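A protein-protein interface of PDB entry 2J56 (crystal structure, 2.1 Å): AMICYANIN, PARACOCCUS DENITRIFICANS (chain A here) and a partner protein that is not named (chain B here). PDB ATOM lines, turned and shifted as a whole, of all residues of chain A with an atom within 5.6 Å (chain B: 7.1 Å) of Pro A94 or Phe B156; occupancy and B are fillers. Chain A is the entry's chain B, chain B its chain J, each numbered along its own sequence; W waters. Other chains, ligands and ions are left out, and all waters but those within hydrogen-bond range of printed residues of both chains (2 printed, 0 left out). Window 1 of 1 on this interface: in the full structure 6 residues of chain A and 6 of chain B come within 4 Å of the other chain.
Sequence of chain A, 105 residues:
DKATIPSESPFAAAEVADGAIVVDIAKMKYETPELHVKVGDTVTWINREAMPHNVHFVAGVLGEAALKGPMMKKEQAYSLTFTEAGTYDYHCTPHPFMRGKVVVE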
ATOM      1  N   PRO A  52     -10.766   8.027 -13.943  1.00  0.00           N
ATOM      2  CA  PRO A  52     -10.801   9.315 -13.242  1.00  0.00           C
ATOM      3  C   PRO A  52     -12.220   9.849 -13.022  1.00  0.00           C
ATOM      4  O   PRO A  52     -13.096   9.721 -13.897  1.00  0.00           O
ATOM      5  CB  PRO A  52      -9.979  10.240 -14.169  1.00  0.00           C
ATOM      6  CG  PRO A  52      -9.105   9.250 -14.957  1.00  0.00           C
ATOM      7  CD  PRO A  52     -10.093   8.143 -15.245  1.00  0.00           C
ATOM      8  N   ASN A  54     -14.496  13.251 -10.882  1.00  0.00           N
ATOM      9  CA  ASN A  54     -14.489  14.432 -10.013  1.00  0.00           C
ATOM     10  C   ASN A  54     -15.879  14.653  -9.456  1.00  0.00           C
ATOM     11  O   ASN A  54     -16.770  13.794  -9.600  1.00  0.00           O
ATOM     12  CB  ASN A  54     -14.000  15.702 -10.761  1.00  0.00           C
ATOM     13  CG  ASN A  54     -14.987  16.185 -11.793  1.00  0.00           C
ATOM     14  OD1 ASN A  54     -15.889  15.442 -12.211  1.00  0.00           O
ATOM     15  ND2 ASN A  54     -14.841  17.450 -12.209  1.00  0.00           N
ATOM     16  N   MET A  71     -10.068  16.354 -11.575  1.00  0.00           N
ATOM     17  CA  MET A  71     -10.169  14.904 -11.749  1.00  0.00           C
ATOM     18  C   MET A  71      -9.226  14.167 -10.777  1.00  0.00           C
ATOM     19  O   MET A  71      -8.052  14.542 -10.594  1.00  0.00           O
ATOM     20  CB  MET A  71      -9.833  14.480 -13.177  1.00  0.00           C
ATOM     21  CG  MET A  71     -10.735  15.057 -14.259  1.00  0.00           C
ATOM     22  SD  MET A  71     -12.534  14.759 -14.029  1.00  0.00           S
ATOM     23  CE  MET A  71     -12.668  13.041 -14.506  1.00  0.00           C
ATOM     24  N   CYS A  92     -20.344  14.112 -12.066  1.00  0.00           N
ATOM     25  CA  CYS A  92     -18.975  13.889 -12.485  1.00  0.00           C
ATOM     26  C   CYS A  92     -18.836  14.363 -13.932  1.00  0.00           C
ATOM     27  O   CYS A  92     -19.572  13.937 -14.837  1.00  0.00           O
ATOM     28  CB  CYS A  92     -18.590  12.420 -12.351  1.00  0.00           C
ATOM     29  SG  CYS A  92     -16.955  12.097 -12.982  1.00  0.00           S
ATOM     30  N   THR A  93     -17.912  15.292 -14.138  1.00  0.00           N
ATOM     31  CA  THR A  93     -17.915  16.061 -15.420  1.00  0.00           C
ATOM     32  C   THR A  93     -18.075  15.221 -16.696  1.00  0.00           C
ATOM     33  O   THR A  93     -18.961  15.508 -17.475  1.00  0.00           O
ATOM     34  CB  THR A  93     -16.747  17.020 -15.527  1.00  0.00           C
ATOM     35  OG1 THR A  93     -16.740  17.905 -14.403  1.00  0.00           O
ATOM     36  CG2 THR A  93     -16.805  17.838 -16.812  1.00  0.00           C
ATOM     37  N   PRO A  94     -17.233  14.184 -16.921  1.00  0.00           N
ATOM     38  CA  PRO A  94     -17.437  13.358 -18.111  1.00  0.00           C
ATOM     39  C   PRO A  94     -18.556  12.321 -17.993  1.00  0.00           C
ATOM     40  O   PRO A  94     -18.887  11.682 -19.001  1.00  0.00           O
ATOM     41  CB  PRO A  94     -16.142  12.580 -18.188  1.00  0.00           C
ATOM     42  CG  PRO A  94     -15.759  12.403 -16.793  1.00  0.00           C
ATOM     43  CD  PRO A  94     -16.055  13.721 -16.163  1.00  0.00           C
ATOM     44  N   HIS A  95     -19.071  12.105 -16.772  1.00  0.00           N
ATOM     45  CA  HIS A  95     -20.054  11.043 -16.518  1.00  0.00           C
ATOM     46  C   HIS A  95     -21.288  11.592 -15.837  1.00  0.00           C
ATOM     47  O   HIS A  95     -21.479  11.415 -14.629  1.00  0.00           O
ATOM     48  CB  HIS A  95     -19.502   9.931 -15.646  1.00  0.00           C
ATOM     49  CG  HIS A  95     -18.128   9.477 -16.016  1.00  0.00           C
ATOM     50  ND1 HIS A  95     -17.175   9.209 -15.061  1.00  0.00           N
ATOM     51  CD2 HIS A  95     -17.546   9.250 -17.221  1.00  0.00           C
ATOM     52  CE1 HIS A  95     -16.047   8.863 -15.661  1.00  0.00           C
ATOM     53  NE2 HIS A  95     -16.249   8.877 -16.975  1.00  0.00           N
ATOM     54  N   PRO A  96     -22.139  12.270 -16.609  1.00  0.00           N
ATOM     55  CA  PRO A  96     -23.315  12.950 -16.072  1.00  0.00           C
ATOM     56  C   PRO A  96     -24.293  11.989 -15.408  1.00  0.00           C
ATOM     57  O   PRO A  96     -25.148  12.437 -14.633  1.00  0.00           O
ATOM     58  CB  PRO A  96     -23.975  13.562 -17.313  1.00  0.00           C
ATOM     59  CG  PRO A  96     -22.921  13.605 -18.331  1.00  0.00           C
ATOM     60  CD  PRO A  96     -22.021  12.429 -18.060  1.00  0.00           C
ATOM     61  N   PHE A  97     -24.168  10.692 -15.733  1.00  0.00           N
ATOM     62  CA  PHE A  97     -24.926   9.616 -15.062  1.00  0.00           C
ATOM     63  C   PHE A  97     -24.466   9.331 -13.623  1.00  0.00           C
ATOM     64  O   PHE A  97     -25.133   8.568 -12.906  1.00  0.00           O
ATOM     65  CB  PHE A  97     -24.859   8.322 -15.892  1.00  0.00           C
ATOM     66  CG  PHE A  97     -23.458   7.882 -16.188  1.00  0.00           C
ATOM     67  CD1 PHE A  97     -22.771   7.060 -15.293  1.00  0.00           C
ATOM     68  CD2 PHE A  97     -22.806   8.323 -17.349  1.00  0.00           C
ATOM     69  CE1 PHE A  97     -21.473   6.681 -15.564  1.00  0.00           C
ATOM     70  CE2 PHE A  97     -21.509   7.942 -17.625  1.00  0.00           C
ATOM     71  CZ  PHE A  97     -20.837   7.127 -16.722  1.00  0.00           C
ATOM     72  N   PRO B 131     -27.785  23.837 -25.437  1.00  0.00           N
ATOM     73  CA  PRO B 131     -28.119  22.496 -24.912  1.00  0.00           C
ATOM     74  C   PRO B 131     -27.844  21.299 -25.854  1.00  0.00           C
ATOM     75  O   PRO B 131     -28.021  20.137 -25.423  1.00  0.00           O
ATOM     76  CB  PRO B 131     -29.621  22.614 -24.646  1.00  0.00           C
ATOM     77  CG  PRO B 131     -30.092  23.526 -25.836  1.00  0.00           C
ATOM     78  CD  PRO B 131     -28.929  24.469 -26.115  1.00  0.00           C
ATOM     79  N   ARG B 132     -27.419  21.535 -27.098  1.00  0.00           N
ATOM     80  CA  ARG B 132     -27.158  20.415 -28.011  1.00  0.00           C
ATOM     81  C   ARG B 132     -25.978  19.552 -27.553  1.00  0.00           C
ATOM     82  O   ARG B 132     -25.014  20.063 -27.020  1.00  0.00           O
ATOM     83  CB  ARG B 132     -26.898  20.866 -29.465  1.00  0.00           C
ATOM     84  CG  ARG B 132     -27.987  21.740 -30.110  1.00  0.00           C
ATOM     85  CD  ARG B 132     -27.704  21.936 -31.634  1.00  0.00           C
ATOM     86  NE  ARG B 132     -27.476  20.609 -32.247  1.00  0.00           N
ATOM     87  CZ  ARG B 132     -26.395  20.223 -32.918  1.00  0.00           C
ATOM     88  NH1 ARG B 132     -25.376  21.070 -33.154  1.00  0.00           N
ATOM     89  NH2 ARG B 132     -26.342  18.972 -33.368  1.00  0.00           N
ATOM     90  N   PHE B 133     -26.089  18.242 -27.797  1.00  0.00           N
ATOM     91  CA  PHE B 133     -25.059  17.256 -27.583  1.00  0.00           C
ATOM     92  C   PHE B 133     -24.150  17.285 -28.800  1.00  0.00           C
ATOM     93  O   PHE B 133     -24.578  16.973 -29.916  1.00  0.00           O
ATOM     94  CB  PHE B 133     -25.707  15.851 -27.472  1.00  0.00           C
ATOM     95  CG  PHE B 133     -24.741  14.720 -27.139  1.00  0.00           C
ATOM     96  CD1 PHE B 133     -23.483  14.958 -26.576  1.00  0.00           C
ATOM     97  CD2 PHE B 133     -25.134  13.397 -27.331  1.00  0.00           C
ATOM     98  CE1 PHE B 133     -22.633  13.900 -26.218  1.00  0.00           C
ATOM     99  CE2 PHE B 133     -24.291  12.332 -26.976  1.00  0.00           C
ATOM    100  CZ  PHE B 133     -23.040  12.583 -26.425  1.00  0.00           C
ATOM    101  N   LEU B 134     -22.895  17.644 -28.575  1.00  0.00           N
ATOM    102  CA  LEU B 134     -21.911  17.694 -29.648  1.00  0.00           C
ATOM    103  C   LEU B 134     -21.172  16.368 -29.722  1.00  0.00           C
ATOM    104  O   LEU B 134     -20.336  16.032 -28.858  1.00  0.00           O
ATOM    105  CB  LEU B 134     -20.964  18.879 -29.411  1.00  0.00           C
ATOM    106  CG  LEU B 134     -21.700  20.220 -29.471  1.00  0.00           C
ATOM    107  CD1 LEU B 134     -20.794  21.419 -29.094  1.00  0.00           C
ATOM    108  CD2 LEU B 134     -22.336  20.419 -30.851  1.00  0.00           C
ATOM    109  N   MET B 141     -30.241  11.117 -32.450  1.00  0.00           N
ATOM    110  CA  MET B 141     -30.053  12.100 -31.367  1.00  0.00           C
ATOM    111  C   MET B 141     -30.911  13.350 -31.551  1.00  0.00           C
ATOM    112  O   MET B 141     -30.929  14.227 -30.681  1.00  0.00           O
ATOM    113  CB  MET B 141     -28.579  12.453 -31.176  1.00  0.00           C
ATOM    114  CG  MET B 141     -27.822  11.361 -30.490  1.00  0.00           C
ATOM    115  SD  MET B 141     -28.288  11.219 -28.767  1.00  0.00           S
ATOM    116  CE  MET B 141     -27.074  10.020 -28.230  1.00  0.00           C
ATOM    117  N   TYR B 154     -31.398  15.645 -27.982  1.00  0.00           N
ATOM    118  CA  TYR B 154     -30.730  15.151 -26.779  1.00  0.00           C
ATOM    119  C   TYR B 154     -29.688  16.138 -26.256  1.00  0.00           C
ATOM    120  O   TYR B 154     -28.897  16.700 -27.027  1.00  0.00           O
ATOM    121  CB  TYR B 154     -30.112  13.759 -27.041  1.00  0.00           C
ATOM    122  CG  TYR B 154     -29.547  13.112 -25.793  1.00  0.00           C
ATOM    123  CD1 TYR B 154     -30.405  12.637 -24.774  1.00  0.00           C
ATOM    124  CD2 TYR B 154     -28.171  12.954 -25.620  1.00  0.00           C
ATOM    125  CE1 TYR B 154     -29.900  12.050 -23.623  1.00  0.00           C
ATOM    126  CE2 TYR B 154     -27.655  12.366 -24.453  1.00  0.00           C
ATOM    127  CZ  TYR B 154     -28.538  11.913 -23.459  1.00  0.00           C
ATOM    128  OH  TYR B 154     -28.034  11.344 -22.298  1.00  0.00           O
ATOM    129  N   GLN B 155     -29.703  16.321 -24.944  1.00  0.00           N
ATOM    130  CA  GLN B 155     -28.624  16.962 -24.201  1.00  0.00           C
ATOM    131  C   GLN B 155     -27.964  15.904 -23.326  1.00  0.00           C
ATOM    132  O   GLN B 155     -28.658  15.151 -22.621  1.00  0.00           O
ATOM    133  CB  GLN B 155     -29.158  18.085 -23.314  1.00  0.00           C
ATOM    134  CG  GLN B 155     -28.115  18.699 -22.356  1.00  0.00           C
ATOM    135  CD  GLN B 155     -28.746  19.630 -21.363  1.00  0.00           C
ATOM    136  OE1 GLN B 155     -29.040  20.786 -21.701  1.00  0.00           O
ATOM    137  NE2 GLN B 155     -28.966  19.142 -20.103  1.00  0.00           N
ATOM    138  N   PHE B 156     -26.628  15.879 -23.350  1.00  0.00           N
ATOM    139  CA  PHE B 156     -25.812  14.913 -22.608  1.00  0.00           C
ATOM    140  C   PHE B 156     -25.378  15.494 -21.271  1.00  0.00           C
ATOM    141  O   PHE B 156     -25.426  14.841 -20.225  1.00  0.00           O
ATOM    142  CB  PHE B 156     -24.590  14.544 -23.460  1.00  0.00           C
ATOM    143  CG  PHE B 156     -23.585  13.639 -22.754  1.00  0.00           C
ATOM    144  CD1 PHE B 156     -23.893  12.298 -22.471  1.00  0.00           C
ATOM    145  CD2 PHE B 156     -22.334  14.126 -22.395  1.00  0.00           C
ATOM    146  CE1 PHE B 156     -22.976  11.465 -21.832  1.00  0.00           C
ATOM    147  CE2 PHE B 156     -21.391  13.305 -21.742  1.00  0.00           C
ATOM    148  CZ  PHE B 156     -21.727  11.978 -21.451  1.00  0.00           C
ATOM    149  N   SER B 157     -24.973  16.759 -21.325  1.00  0.00           N
ATOM    150  CA  SER B 157     -24.368  17.410 -20.222  1.00  0.00           C
ATOM    151  C   SER B 157     -24.828  18.856 -19.941  1.00  0.00           C
ATOM    152  O   SER B 157     -25.203  19.554 -20.880  1.00  0.00           O
ATOM    153  CB  SER B 157     -22.840  17.485 -20.508  1.00  0.00           C
ATOM    154  OG  SER B 157     -22.200  18.365 -19.588  1.00  0.00           O
ATOM    155  N   PRO B 158     -25.191  19.134 -18.694  1.00  0.00           N
ATOM    156  CA  PRO B 158     -24.576  18.779 -17.429  1.00  0.00           C
ATOM    157  C   PRO B 158     -25.391  17.534 -16.920  1.00  0.00           C
ATOM    158  O   PRO B 158     -24.956  16.833 -16.034  1.00  0.00           O
ATOM    159  CB  PRO B 158     -24.816  19.996 -16.543  1.00  0.00           C
ATOM    160  CG  PRO B 158     -26.044  20.666 -17.098  1.00  0.00           C
ATOM    161  CD  PRO B 158     -25.953  20.401 -18.595  1.00  0.00           C
ATOM    162  N   ALA B 159     -26.560  17.264 -17.486  1.00  0.00           N
ATOM    163  CA  ALA B 159     -27.412  16.153 -17.026  1.00  0.00           C
ATOM    164  C   ALA B 159     -28.211  15.670 -18.236  1.00  0.00           C
ATOM    165  O   ALA B 159     -28.437  16.448 -19.153  1.00  0.00           O
ATOM    166  CB  ALA B 159     -28.367  16.623 -15.903  1.00  0.00           C
ATOM    167  N   PRO B 160     -28.667  14.395 -18.236  1.00  0.00           N
ATOM    168  CA  PRO B 160     -29.403  13.910 -19.420  1.00  0.00           C
ATOM    169  C   PRO B 160     -30.738  14.647 -19.571  1.00  0.00           C
ATOM    170  O   PRO B 160     -31.469  14.832 -18.584  1.00  0.00           O
ATOM    171  CB  PRO B 160     -29.641  12.425 -19.112  1.00  0.00           C
ATOM    172  CG  PRO B 160     -29.568  12.310 -17.649  1.00  0.00           C
ATOM    173  CD  PRO B 160     -28.568  13.367 -17.177  1.00  0.00           C
ATOM    174  N   ALA B 161     -31.075  15.080 -20.777  1.00  0.00           N
ATOM    175  CA  ALA B 161     -32.315  15.826 -20.933  1.00  0.00           C
ATOM    176  C   ALA B 161     -32.739  15.811 -22.363  1.00  0.00           C
ATOM    177  O   ALA B 161     -31.944  15.467 -23.246  1.00  0.00           O
ATOM    178  CB  ALA B 161     -32.187  17.261 -20.430  1.00  0.00           C
ATOM    179  N   ASP B 180     -30.707   8.374 -17.289  1.00  0.00           N
ATOM    180  CA  ASP B 180     -29.473   8.121 -18.010  1.00  0.00           C
ATOM    181  C   ASP B 180     -29.662   7.211 -19.222  1.00  0.00           C
ATOM    182  O   ASP B 180     -29.191   6.071 -19.251  1.00  0.00           O
ATOM    183  CB  ASP B 180     -28.455   7.594 -17.049  1.00  0.00           C
ATOM    184  CG  ASP B 180     -28.180   8.569 -15.976  1.00  0.00           C
ATOM    185  OD1 ASP B 180     -27.765   9.696 -16.350  1.00  0.00           O
ATOM    186  OD2 ASP B 180     -28.376   8.243 -14.773  1.00  0.00           O
ATOM    187  N   CYS B 181     -30.324   7.768 -20.230  1.00  0.00           N
ATOM    188  CA  CYS B 181     -30.625   7.087 -21.489  1.00  0.00           C
ATOM    189  C   CYS B 181     -30.170   7.995 -22.639  1.00  0.00           C
ATOM    190  O   CYS B 181     -29.790   9.149 -22.399  1.00  0.00           O
ATOM    191  CB  CYS B 181     -32.134   6.769 -21.566  1.00  0.00           C
ATOM    192  SG  CYS B 181     -32.766   6.021 -19.982  1.00  0.00           S
ATOM    193  N   TYR B 182     -30.240   7.488 -23.867  1.00  0.00           N
ATOM    194  CA  TYR B 182     -29.522   8.035 -25.055  1.00  0.00           C
ATOM    195  C   TYR B 182     -30.350   7.667 -26.248  1.00  0.00           C
ATOM    196  O   TYR B 182     -30.918   6.556 -26.247  1.00  0.00           O
ATOM    197  CB  TYR B 182     -28.136   7.370 -25.180  1.00  0.00           C
ATOM    198  CG  TYR B 182     -27.361   7.587 -23.914  1.00  0.00           C
ATOM    199  CD1 TYR B 182     -27.440   6.674 -22.875  1.00  0.00           C
ATOM    200  CD2 TYR B 182     -26.621   8.754 -23.717  1.00  0.00           C
ATOM    201  CE1 TYR B 182     -26.789   6.891 -21.658  1.00  0.00           C
ATOM    202  CE2 TYR B 182     -25.955   8.987 -22.492  1.00  0.00           C
ATOM    203  CZ  TYR B 182     -26.045   8.034 -21.474  1.00  0.00           C
ATOM    204  OH  TYR B 182     -25.412   8.217 -20.257  1.00  0.00           O
HETATM  205  O   HOH W   1     -20.393  17.660 -17.518  1.00  0.00           O
HETATM  206  O   HOH W   2     -25.795  15.080 -14.150  1.00  0.00           O
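Among the printed residues, merely in contact across the chains: Phe A97 with Asp B180 (3.1 Å), Pro A96 with Phe B156 (3.4 Å), Pro A96 with Pro B158 (3.6 Å), Pro A94 with Phe B156 (3.8 Å) and Phe A97 with Tyr B182 (3.9 Å).
Pro A94 touches just one residue of chain B: Phe B156. Phe B156 touches just these residues of chain A: Pro A94 and Pro A96. Of the printed residues of chain B, Phe A97 touches Asp B180 and Tyr B182. Of the printed residues of chain A, Asp B180 touches Phe A97 (3.1 Å). Of the printed residues of chain A, Pro B158 touches Pro A96 (3.6 Å). Printed residues of chain B within 4 Å of Pro A96: Phe B156 (3.4 Å) and Pro B158 (3.6 Å). Of the printed residues of chain A, Tyr B182 touches Phe A97. The nearest residue of chain B that does not touch Pro A94 is Ser B157 (7.0 Å). The nearest printed residue of chain A that does not touch Pro B158 is Phe A97 (6.2 Å).
Of the 16 printed residues of chain B, 4 touch a printed residue of chain A. Among the printed residues, no Asp or Glu carboxylate lies within 4 Å of a Lys or Arg side-chain nitrogen of the other chain.
Water W1 bridges the backbone carbonyl oxygen of Thr A93 (2.6 Å) and the side-chain hydroxyl of Ser B157 (2.8 Å). Water W2 bridges the backbone carbonyl oxygen of Pro B158 (2.7 Å) and the backbone carbonyl oxygen of Pro A96 (2.8 Å).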
